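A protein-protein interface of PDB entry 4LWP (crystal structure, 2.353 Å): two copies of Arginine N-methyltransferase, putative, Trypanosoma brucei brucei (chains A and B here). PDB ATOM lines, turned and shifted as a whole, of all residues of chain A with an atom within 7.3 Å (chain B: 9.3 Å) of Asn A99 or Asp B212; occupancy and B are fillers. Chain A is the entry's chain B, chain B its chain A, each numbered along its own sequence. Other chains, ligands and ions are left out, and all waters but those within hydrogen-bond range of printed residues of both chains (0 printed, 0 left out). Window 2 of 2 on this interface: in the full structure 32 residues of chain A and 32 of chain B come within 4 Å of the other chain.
The side-chain amide oxygen (OD1) of Asn A99 sits at hydrogen-bond distance from the backbone NH (N) of Asp B212 (2.9 Å).
OD2 of Asp A98 is in salt-bridge range of NE of Arg B215 (2.5 Å).
The side-chain carboxylate (OD1) of Asp B212 is in hydrogen-bond range of the side-chain hydroxyl (OG) of Ser B214 (2.6 Å).
The side-chain amide nitrogen of Asn A99 sits at hydrogen-bond distance from the backbone carbonyl oxygen of Val A95, 2.7 Å away.
The backbone NH (N) of Phe B213 lies within hydrogen-bond range of the backbone carbonyl oxygen (O) of Trp B205 (3.0 Å).
Met A70 touches Leu B211.
SD of Met A70 touches CE1 of Phe B213, at 3.9 Å.
Gln A92 touches Tyr B216 (CA to OH, 3.2 Å).
Arg B215 touches Gly A94.
Val A95 touches Asp B212.
Phe B213 touches Val A95 (CD1 to CG1, 3.6 Å).
Arg B215 touches Val A95.
Val A95 touches Tyr B216 (CG2 to CZ, 3.4 Å).
Leu B211 touches Asn A99.
Of chain B, only Leu B211 (3.4 Å) and Asp B212 (2.9 Å) come within 4 Å of Asn A99.
Printed residues of chain A within 4 Å of Leu B211: Met A70 (3.6 Å) and Asn A99 (3.4 Å).
Printed residues of chain A within 4 Å of Phe B213: Met A70 (3.9 Å) and Val A95 (3.6 Å).
The nearest residue of chain A that does not touch Asp B212 is Asp A98 (4.3 Å).
The nearest printed residue of chain A that does not touch Tyr B216 is Met A70 (4.8 Å).
Of the 12 printed residues of chain A, 6 touch a printed residue of chain B.
Printed residues of chain A that touch a printed residue of chain B: Met A70, Gln A92, Gly A94, Val A95, Asp A98 and Asn A99.
Hydrophobic or aromatic side chains of chain A within 4 Å of the printed part of chain B: Met A70 and Val A95.
Along chain A the printed residues that touch a printed residue of chain B span positions 70 to 99.
Of the 18 printed residues of chain B, 5 touch a printed residue of chain A.
Printed residues of chain B that touch a printed residue of chain A: Leu B211, Asp B212, Phe B213, Arg B215 and Tyr B216.
Hydrophobic or aromatic side chains of chain B that line the printed part of chain A: Leu B211, Phe B213 and Tyr B216.
Among the printed residues, 11 pairs touch across the chains.
Among the printed residues, Asp or Glu carboxylates within 4 Å of a Lys or Arg side-chain nitrogen of the other chain: Asp A98 with Arg B215.
No position is printed for both chains.
Of the 11 pairs that touch across the chains among the printed residues, none has its exchanged pair printed and touching as well.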
ATOM      1  N   MET A  70       6.501  -2.271  21.077  1.00  0.00           N
ATOM      2  CA  MET A  70       5.736  -1.910  22.267  1.00  0.00           C
ATOM      3  C   MET A  70       4.520  -2.833  22.491  1.00  0.00           C
ATOM      4  O   MET A  70       4.188  -3.157  23.647  1.00  0.00           O
ATOM      5  CB  MET A  70       5.322  -0.435  22.170  1.00  0.00           C
ATOM      6  CG  MET A  70       6.453   0.508  22.624  1.00  0.00           C
ATOM      7  SD  MET A  70       6.230   2.245  22.205  1.00  0.00           S
ATOM      8  CE  MET A  70       7.429   2.473  20.900  1.00  0.00           C
ATOM      9  N   GLN A  92      12.376   7.082  19.198  1.00  0.00           N
ATOM     10  CA  GLN A  92      11.728   5.877  19.731  1.00  0.00           C
ATOM     11  C   GLN A  92      12.216   5.571  21.146  1.00  0.00           C
ATOM     12  O   GLN A  92      11.452   5.085  21.984  1.00  0.00           O
ATOM     13  CB  GLN A  92      11.965   4.665  18.809  1.00  0.00           C
ATOM     14  CG  GLN A  92      11.145   3.433  19.210  1.00  0.00           C
ATOM     15  CD  GLN A  92      11.493   2.185  18.406  1.00  0.00           C
ATOM     16  OE1 GLN A  92      11.698   2.255  17.195  1.00  0.00           O
ATOM     17  NE2 GLN A  92      11.539   1.036  19.076  1.00  0.00           N
ATOM     18  N   ILE A  93      13.487   5.864  21.415  1.00  0.00           N
ATOM     19  CA  ILE A  93      14.008   5.723  22.778  1.00  0.00           C
ATOM     20  C   ILE A  93      13.177   6.584  23.736  1.00  0.00           C
ATOM     21  O   ILE A  93      12.714   6.095  24.772  1.00  0.00           O
ATOM     22  CB  ILE A  93      15.509   6.103  22.868  1.00  0.00           C
ATOM     23  CG1 ILE A  93      16.351   5.063  22.128  1.00  0.00           C
ATOM     24  CG2 ILE A  93      15.961   6.161  24.309  1.00  0.00           C
ATOM     25  CD1 ILE A  93      17.773   5.486  21.872  1.00  0.00           C
ATOM     26  N   GLY A  94      12.935   7.844  23.363  1.00  0.00           N
ATOM     27  CA  GLY A  94      12.092   8.719  24.173  1.00  0.00           C
ATOM     28  C   GLY A  94      10.675   8.207  24.360  1.00  0.00           C
ATOM     29  O   GLY A  94      10.180   8.161  25.484  1.00  0.00           O
ATOM     30  N   VAL A  95      10.028   7.781  23.274  1.00  0.00           N
ATOM     31  CA  VAL A  95       8.647   7.289  23.355  1.00  0.00           C
ATOM     32  C   VAL A  95       8.552   5.986  24.148  1.00  0.00           C
ATOM     33  O   VAL A  95       7.548   5.730  24.836  1.00  0.00           O
ATOM     34  CB  VAL A  95       8.040   7.073  21.942  1.00  0.00           C
ATOM     35  CG1 VAL A  95       6.647   6.453  22.015  1.00  0.00           C
ATOM     36  CG2 VAL A  95       7.989   8.382  21.203  1.00  0.00           C
ATOM     37  N   VAL A  96       9.577   5.145  24.047  1.00  0.00           N
ATOM     38  CA  VAL A  96       9.603   3.946  24.885  1.00  0.00           C
ATOM     39  C   VAL A  96       9.672   4.338  26.373  1.00  0.00           C
ATOM     40  O   VAL A  96       8.940   3.792  27.219  1.00  0.00           O
ATOM     41  CB  VAL A  96      10.783   3.019  24.521  1.00  0.00           C
ATOM     42  CG1 VAL A  96      10.989   1.960  25.613  1.00  0.00           C
ATOM     43  CG2 VAL A  96      10.518   2.330  23.182  1.00  0.00           C
ATOM     44  N   GLU A  97      10.515   5.319  26.673  1.00  0.00           N
ATOM     45  CA  GLU A  97      10.605   5.858  28.023  1.00  0.00           C
ATOM     46  C   GLU A  97       9.288   6.518  28.436  1.00  0.00           C
ATOM     47  O   GLU A  97       8.796   6.266  29.540  1.00  0.00           O
ATOM     48  CB  GLU A  97      11.762   6.859  28.131  1.00  0.00           C
ATOM     49  CG  GLU A  97      11.819   7.618  29.458  1.00  0.00           C
ATOM     50  CD  GLU A  97      11.869   6.686  30.662  1.00  0.00           C
ATOM     51  OE1 GLU A  97      12.713   5.757  30.662  1.00  0.00           O
ATOM     52  OE2 GLU A  97      11.057   6.872  31.601  1.00  0.00           O
ATOM     53  N   ASP A  98       8.697   7.315  27.539  1.00  0.00           N
ATOM     54  CA  ASP A  98       7.397   7.959  27.816  1.00  0.00           C
ATOM     55  C   ASP A  98       6.305   6.945  28.120  1.00  0.00           C
ATOM     56  O   ASP A  98       5.341   7.272  28.805  1.00  0.00           O
ATOM     57  CB  ASP A  98       6.931   8.841  26.639  1.00  0.00           C
ATOM     58  CG  ASP A  98       7.895   9.971  26.329  1.00  0.00           C
ATOM     59  OD1 ASP A  98       8.608  10.430  27.248  1.00  0.00           O
ATOM     60  OD2 ASP A  98       7.962  10.402  25.157  1.00  0.00           O
ATOM     61  N   ASN A  99       6.463   5.711  27.652  1.00  0.00           N
ATOM     62  CA  ASN A  99       5.469   4.671  27.938  1.00  0.00           C
ATOM     63  C   ASN A  99       5.958   3.674  28.984  1.00  0.00           C
ATOM     64  O   ASN A  99       5.409   2.568  29.105  1.00  0.00           O
ATOM     65  CB  ASN A  99       5.070   3.921  26.667  1.00  0.00           C
ATOM     66  CG  ASN A  99       4.214   4.752  25.751  1.00  0.00           C
ATOM     67  OD1 ASN A  99       2.983   4.688  25.811  1.00  0.00           O
ATOM     68  ND2 ASN A  99       4.852   5.549  24.904  1.00  0.00           N
ATOM     69  N   ASP A 100       7.000   4.069  29.717  1.00  0.00           N
ATOM     70  CA  ASP A 100       7.490   3.300  30.861  1.00  0.00           C
ATOM     71  C   ASP A 100       7.889   1.887  30.458  1.00  0.00           C
ATOM     72  O   ASP A 100       7.545   0.931  31.154  1.00  0.00           O
ATOM     73  CB  ASP A 100       6.425   3.243  31.970  1.00  0.00           C
ATOM     74  CG  ASP A 100       6.141   4.605  32.580  1.00  0.00           C
ATOM     75  N   LEU A 101       8.604   1.745  29.342  1.00  0.00           N
ATOM     76  CA  LEU A 101       8.938   0.409  28.840  1.00  0.00           C
ATOM     77  C   LEU A 101      10.427   0.243  28.596  1.00  0.00           C
ATOM     78  O   LEU A 101      10.849  -0.699  27.919  1.00  0.00           O
ATOM     79  CB  LEU A 101       8.167   0.104  27.544  1.00  0.00           C
ATOM     80  CG  LEU A 101       6.700  -0.290  27.743  1.00  0.00           C
ATOM     81  CD1 LEU A 101       5.927  -0.394  26.422  1.00  0.00           C
ATOM     82  CD2 LEU A 101       6.616  -1.595  28.497  1.00  0.00           C
ATOM     83  N   SER A 102      11.222   1.148  29.153  1.00  0.00           N
ATOM     84  CA  SER A 102      12.642   1.178  28.846  1.00  0.00           C
ATOM     85  C   SER A 102      13.416  -0.052  29.303  1.00  0.00           C
ATOM     86  O   SER A 102      14.512  -0.298  28.811  1.00  0.00           O
ATOM     87  CB  SER A 102      13.269   2.430  29.433  1.00  0.00           C
ATOM     88  OG  SER A 102      12.761   3.557  28.743  1.00  0.00           O
ATOM     89  N   TYR B 197      -2.447  22.575  15.734  1.00  0.00           N
ATOM     90  CA  TYR B 197      -1.643  21.542  16.345  1.00  0.00           C
ATOM     91  C   TYR B 197      -2.541  20.486  16.966  1.00  0.00           C
ATOM     92  O   TYR B 197      -2.345  19.285  16.749  1.00  0.00           O
ATOM     93  CB  TYR B 197      -0.718  22.121  17.409  1.00  0.00           C
ATOM     94  CG  TYR B 197      -0.114  21.054  18.292  1.00  0.00           C
ATOM     95  CD1 TYR B 197       0.753  20.100  17.769  1.00  0.00           C
ATOM     96  CD2 TYR B 197      -0.433  20.978  19.643  1.00  0.00           C
ATOM     97  CE1 TYR B 197       1.301  19.106  18.573  1.00  0.00           C
ATOM     98  CE2 TYR B 197       0.110  19.983  20.463  1.00  0.00           C
ATOM     99  CZ  TYR B 197       0.975  19.053  19.916  1.00  0.00           C
ATOM    100  OH  TYR B 197       1.522  18.067  20.710  1.00  0.00           O
ATOM    101  N   LYS B 202      -2.029  16.572  17.634  1.00  0.00           N
ATOM    102  CA  LYS B 202      -2.064  16.104  19.005  1.00  0.00           C
ATOM    103  C   LYS B 202      -3.173  15.082  19.217  1.00  0.00           C
ATOM    104  O   LYS B 202      -3.018  14.131  19.969  1.00  0.00           O
ATOM    105  CB  LYS B 202      -2.247  17.278  19.956  1.00  0.00           C
ATOM    106  CG  LYS B 202      -2.314  16.858  21.411  1.00  0.00           C
ATOM    107  CD  LYS B 202      -2.432  18.061  22.313  1.00  0.00           C
ATOM    108  CE  LYS B 202      -2.207  17.665  23.750  1.00  0.00           C
ATOM    109  NZ  LYS B 202      -1.910  18.881  24.554  1.00  0.00           N
ATOM    110  N   ASN B 203      -4.306  15.303  18.570  1.00  0.00           N
ATOM    111  CA  ASN B 203      -5.420  14.378  18.674  1.00  0.00           C
ATOM    112  C   ASN B 203      -5.091  12.977  18.157  1.00  0.00           C
ATOM    113  O   ASN B 203      -5.486  11.999  18.769  1.00  0.00           O
ATOM    114  CB  ASN B 203      -6.637  14.913  17.917  1.00  0.00           C
ATOM    115  CG  ASN B 203      -7.417  15.946  18.708  1.00  0.00           C
ATOM    116  OD1 ASN B 203      -7.224  16.111  19.922  1.00  0.00           O
ATOM    117  ND2 ASN B 203      -8.321  16.638  18.023  1.00  0.00           N
ATOM    118  N   PHE B 204      -4.362  12.874  17.046  1.00  0.00           N
ATOM    119  CA  PHE B 204      -4.014  11.555  16.516  1.00  0.00           C
ATOM    120  C   PHE B 204      -2.904  10.871  17.332  1.00  0.00           C
ATOM    121  O   PHE B 204      -3.001   9.690  17.659  1.00  0.00           O
ATOM    122  CB  PHE B 204      -3.585  11.636  15.049  1.00  0.00           C
ATOM    123  CG  PHE B 204      -2.878  10.400  14.581  1.00  0.00           C
ATOM    124  CD1 PHE B 204      -3.597   9.298  14.149  1.00  0.00           C
ATOM    125  CD2 PHE B 204      -1.488  10.315  14.639  1.00  0.00           C
ATOM    126  CE1 PHE B 204      -2.951   8.139  13.769  1.00  0.00           C
ATOM    127  CE2 PHE B 204      -0.840   9.152  14.258  1.00  0.00           C
ATOM    128  CZ  PHE B 204      -1.574   8.068  13.822  1.00  0.00           C
ATOM    129  N   TRP B 205      -1.842  11.610  17.639  1.00  0.00           N
ATOM    130  CA  TRP B 205      -0.651  11.022  18.234  1.00  0.00           C
ATOM    131  C   TRP B 205      -0.794  10.737  19.732  1.00  0.00           C
ATOM    132  O   TRP B 205       0.032  10.017  20.291  1.00  0.00           O
ATOM    133  CB  TRP B 205       0.563  11.919  17.999  1.00  0.00           C
ATOM    134  CG  TRP B 205       1.056  11.946  16.574  1.00  0.00           C
ATOM    135  CD1 TRP B 205       0.893  12.957  15.673  1.00  0.00           C
ATOM    136  CD2 TRP B 205       1.798  10.917  15.887  1.00  0.00           C
ATOM    137  NE1 TRP B 205       1.487  12.633  14.480  1.00  0.00           N
ATOM    138  CE2 TRP B 205       2.046  11.387  14.582  1.00  0.00           C
ATOM    139  CE3 TRP B 205       2.267   9.645  16.248  1.00  0.00           C
ATOM    140  CZ2 TRP B 205       2.753  10.631  13.635  1.00  0.00           C
ATOM    141  CZ3 TRP B 205       2.959   8.896  15.301  1.00  0.00           C
ATOM    142  CH2 TRP B 205       3.197   9.393  14.016  1.00  0.00           C
ATOM    143  N   ARG B 206      -1.824  11.276  20.384  1.00  0.00           N
ATOM    144  CA  ARG B 206      -1.891  11.190  21.839  1.00  0.00           C
ATOM    145  C   ARG B 206      -2.068   9.770  22.316  1.00  0.00           C
ATOM    146  O   ARG B 206      -1.521   9.403  23.345  1.00  0.00           O
ATOM    147  CB  ARG B 206      -3.061  12.025  22.401  1.00  0.00           C
ATOM    148  CG  ARG B 206      -4.448  11.484  21.996  1.00  0.00           C
ATOM    149  CD  ARG B 206      -5.658  12.227  22.594  1.00  0.00           C
ATOM    150  NE  ARG B 206      -5.862  11.908  24.016  1.00  0.00           N
ATOM    151  CZ  ARG B 206      -6.752  11.014  24.463  1.00  0.00           C
ATOM    152  NH1 ARG B 206      -7.539  10.352  23.611  1.00  0.00           N
ATOM    153  NH2 ARG B 206      -6.866  10.777  25.767  1.00  0.00           N
ATOM    154  N   ASP B 207      -2.789   8.972  21.539  1.00  0.00           N
ATOM    155  CA  ASP B 207      -3.065   7.592  21.887  1.00  0.00           C
ATOM    156  C   ASP B 207      -3.131   6.688  20.672  1.00  0.00           C
ATOM    157  O   ASP B 207      -4.106   6.734  19.908  1.00  0.00           O
ATOM    158  CB  ASP B 207      -4.368   7.467  22.658  1.00  0.00           C
ATOM    159  CG  ASP B 207      -4.589   6.056  23.174  1.00  0.00           C
ATOM    160  OD1 ASP B 207      -5.156   5.229  22.420  1.00  0.00           O
ATOM    161  OD2 ASP B 207      -4.165   5.769  24.325  1.00  0.00           O
ATOM    162  N   VAL B 208      -2.100   5.875  20.485  1.00  0.00           N
ATOM    163  CA  VAL B 208      -2.114   4.901  19.404  1.00  0.00           C
ATOM    164  C   VAL B 208      -2.229   3.537  20.053  1.00  0.00           C
ATOM    165  O   VAL B 208      -1.227   2.987  20.513  1.00  0.00           O
ATOM    166  CB  VAL B 208      -0.849   4.972  18.537  1.00  0.00           C
ATOM    167  CG1 VAL B 208      -0.919   3.939  17.414  1.00  0.00           C
ATOM    168  CG2 VAL B 208      -0.650   6.378  17.995  1.00  0.00           C
ATOM    169  N   ASP B 209      -3.452   3.011  20.117  1.00  0.00           N
ATOM    170  CA  ASP B 209      -3.749   1.817  20.907  1.00  0.00           C
ATOM    171  C   ASP B 209      -3.108   1.838  22.300  1.00  0.00           C
ATOM    172  O   ASP B 209      -2.267   0.991  22.620  1.00  0.00           O
ATOM    173  CB  ASP B 209      -3.325   0.544  20.177  1.00  0.00           C
ATOM    174  CG  ASP B 209      -3.809  -0.719  20.892  1.00  0.00           C
ATOM    175  OD1 ASP B 209      -4.924  -0.703  21.479  1.00  0.00           O
ATOM    176  OD2 ASP B 209      -3.067  -1.727  20.893  1.00  0.00           O
ATOM    177  N   GLY B 210      -3.450   2.842  23.099  1.00  0.00           N
ATOM    178  CA  GLY B 210      -2.995   2.910  24.478  1.00  0.00           C
ATOM    179  C   GLY B 210      -1.586   3.447  24.625  1.00  0.00           C
ATOM    180  O   GLY B 210      -1.147   3.789  25.729  1.00  0.00           O
ATOM    181  N   LEU B 211      -0.885   3.582  23.508  1.00  0.00           N
ATOM    182  CA  LEU B 211       0.453   4.138  23.562  1.00  0.00           C
ATOM    183  C   LEU B 211       0.429   5.650  23.420  1.00  0.00           C
ATOM    184  O   LEU B 211      -0.341   6.206  22.637  1.00  0.00           O
ATOM    185  CB  LEU B 211       1.329   3.507  22.480  1.00  0.00           C
ATOM    186  CG  LEU B 211       1.623   2.022  22.687  1.00  0.00           C
ATOM    187  CD1 LEU B 211       2.277   1.421  21.465  1.00  0.00           C
ATOM    188  CD2 LEU B 211       2.555   1.872  23.888  1.00  0.00           C
ATOM    189  N   ASP B 212       1.279   6.312  24.190  1.00  0.00           N
ATOM    190  CA  ASP B 212       1.412   7.743  24.079  1.00  0.00           C
ATOM    191  C   ASP B 212       2.484   8.077  23.058  1.00  0.00           C
ATOM    192  O   ASP B 212       3.681   8.096  23.379  1.00  0.00           O
ATOM    193  CB  ASP B 212       1.764   8.352  25.428  1.00  0.00           C
ATOM    194  CG  ASP B 212       1.944   9.835  25.348  1.00  0.00           C
ATOM    195  OD1 ASP B 212       1.012  10.492  24.844  1.00  0.00           O
ATOM    196  OD2 ASP B 212       3.009  10.343  25.771  1.00  0.00           O
ATOM    197  N   PHE B 213       2.059   8.372  21.835  1.00  0.00           N
ATOM    198  CA  PHE B 213       3.005   8.708  20.781  1.00  0.00           C
ATOM    199  C   PHE B 213       3.088  10.218  20.612  1.00  0.00           C
ATOM    200  O   PHE B 213       3.500  10.706  19.552  1.00  0.00           O
ATOM    201  CB  PHE B 213       2.602   8.066  19.443  1.00  0.00           C
ATOM    202  CG  PHE B 213       3.045   6.634  19.276  1.00  0.00           C
ATOM    203  CD1 PHE B 213       3.447   5.873  20.360  1.00  0.00           C
ATOM    204  CD2 PHE B 213       3.076   6.061  18.011  1.00  0.00           C
ATOM    205  CE1 PHE B 213       3.858   4.547  20.187  1.00  0.00           C
ATOM    206  CE2 PHE B 213       3.486   4.751  17.828  1.00  0.00           C
ATOM    207  CZ  PHE B 213       3.876   3.985  18.918  1.00  0.00           C
ATOM    208  N   SER B 214       2.687  10.956  21.647  1.00  0.00           N
ATOM    209  CA  SER B 214       2.551  12.404  21.526  1.00  0.00           C
ATOM    210  C   SER B 214       3.885  13.092  21.233  1.00  0.00           C
ATOM    211  O   SER B 214       3.907  14.187  20.663  1.00  0.00           O
ATOM    212  CB  SER B 214       1.901  12.986  22.787  1.00  0.00           C
ATOM    213  OG  SER B 214       2.505  12.488  23.960  1.00  0.00           O
ATOM    214  N   ARG B 215       4.993  12.452  21.606  1.00  0.00           N
ATOM    215  CA  ARG B 215       6.323  12.935  21.217  1.00  0.00           C
ATOM    216  C   ARG B 215       6.522  12.936  19.696  1.00  0.00           C
ATOM    217  O   ARG B 215       7.197  13.809  19.144  1.00  0.00           O
ATOM    218  CB  ARG B 215       7.414  12.080  21.853  1.00  0.00           C
ATOM    219  CG  ARG B 215       8.832  12.567  21.558  1.00  0.00           C
ATOM    220  CD  ARG B 215       9.859  11.610  22.179  1.00  0.00           C
ATOM    221  NE  ARG B 215       9.646  11.494  23.628  1.00  0.00           N
ATOM    222  CZ  ARG B 215      10.179  12.313  24.531  1.00  0.00           C
ATOM    223  NH1 ARG B 215      10.959  13.318  24.138  1.00  0.00           N
ATOM    224  NH2 ARG B 215       9.920  12.132  25.824  1.00  0.00           N
ATOM    225  N   TYR B 216       5.976  11.926  19.026  1.00  0.00           N
ATOM    226  CA  TYR B 216       6.036  11.887  17.576  1.00  0.00           C
ATOM    227  C   TYR B 216       5.216  13.038  17.003  1.00  0.00           C
ATOM    228  O   TYR B 216       5.607  13.647  16.007  1.00  0.00           O
ATOM    229  CB  TYR B 216       5.530  10.539  17.037  1.00  0.00           C
ATOM    230  CG  TYR B 216       6.422   9.365  17.377  1.00  0.00           C
ATOM    231  CD1 TYR B 216       7.797   9.457  17.233  1.00  0.00           C
ATOM    232  CD2 TYR B 216       5.892   8.166  17.837  1.00  0.00           C
ATOM    233  CE1 TYR B 216       8.623   8.399  17.534  1.00  0.00           C
ATOM    234  CE2 TYR B 216       6.720   7.090  18.146  1.00  0.00           C
ATOM    235  CZ  TYR B 216       8.084   7.225  17.991  1.00  0.00           C
ATOM    236  OH  TYR B 216       8.933   6.194  18.284  1.00  0.00           O
ATOM    237  N   GLY B 217       4.107  13.357  17.667  1.00  0.00           N
ATOM    238  CA  GLY B 217       3.248  14.455  17.257  1.00  0.00           C
ATOM    239  C   GLY B 217       3.918  15.811  17.225  1.00  0.00           C
ATOM    240  O   GLY B 217       3.742  16.550  16.251  1.00  0.00           O
ATOM    241  N   ARG B 218       4.683  16.144  18.266  1.00  0.00           N
ATOM    242  CA  ARG B 218       5.429  17.402  18.268  1.00  0.00           C
ATOM    243  C   ARG B 218       6.448  17.454  17.154  1.00  0.00           C
ATOM    244  O   ARG B 218       6.545  18.446  16.431  1.00  0.00           O
ATOM    245  CB  ARG B 218       6.118  17.621  19.606  1.00  0.00           C
ATOM    246  CG  ARG B 218       5.137  17.843  20.730  1.00  0.00           C
ATOM    247  CD  ARG B 218       5.836  18.161  22.031  1.00  0.00           C
ATOM    248  NE  ARG B 218       5.830  16.994  22.898  1.00  0.00           N
ATOM    249  CZ  ARG B 218       4.754  16.592  23.572  1.00  0.00           C
ATOM    250  NH1 ARG B 218       3.597  17.257  23.446  1.00  0.00           N
ATOM    251  NH2 ARG B 218       4.826  15.519  24.354  1.00  0.00           N
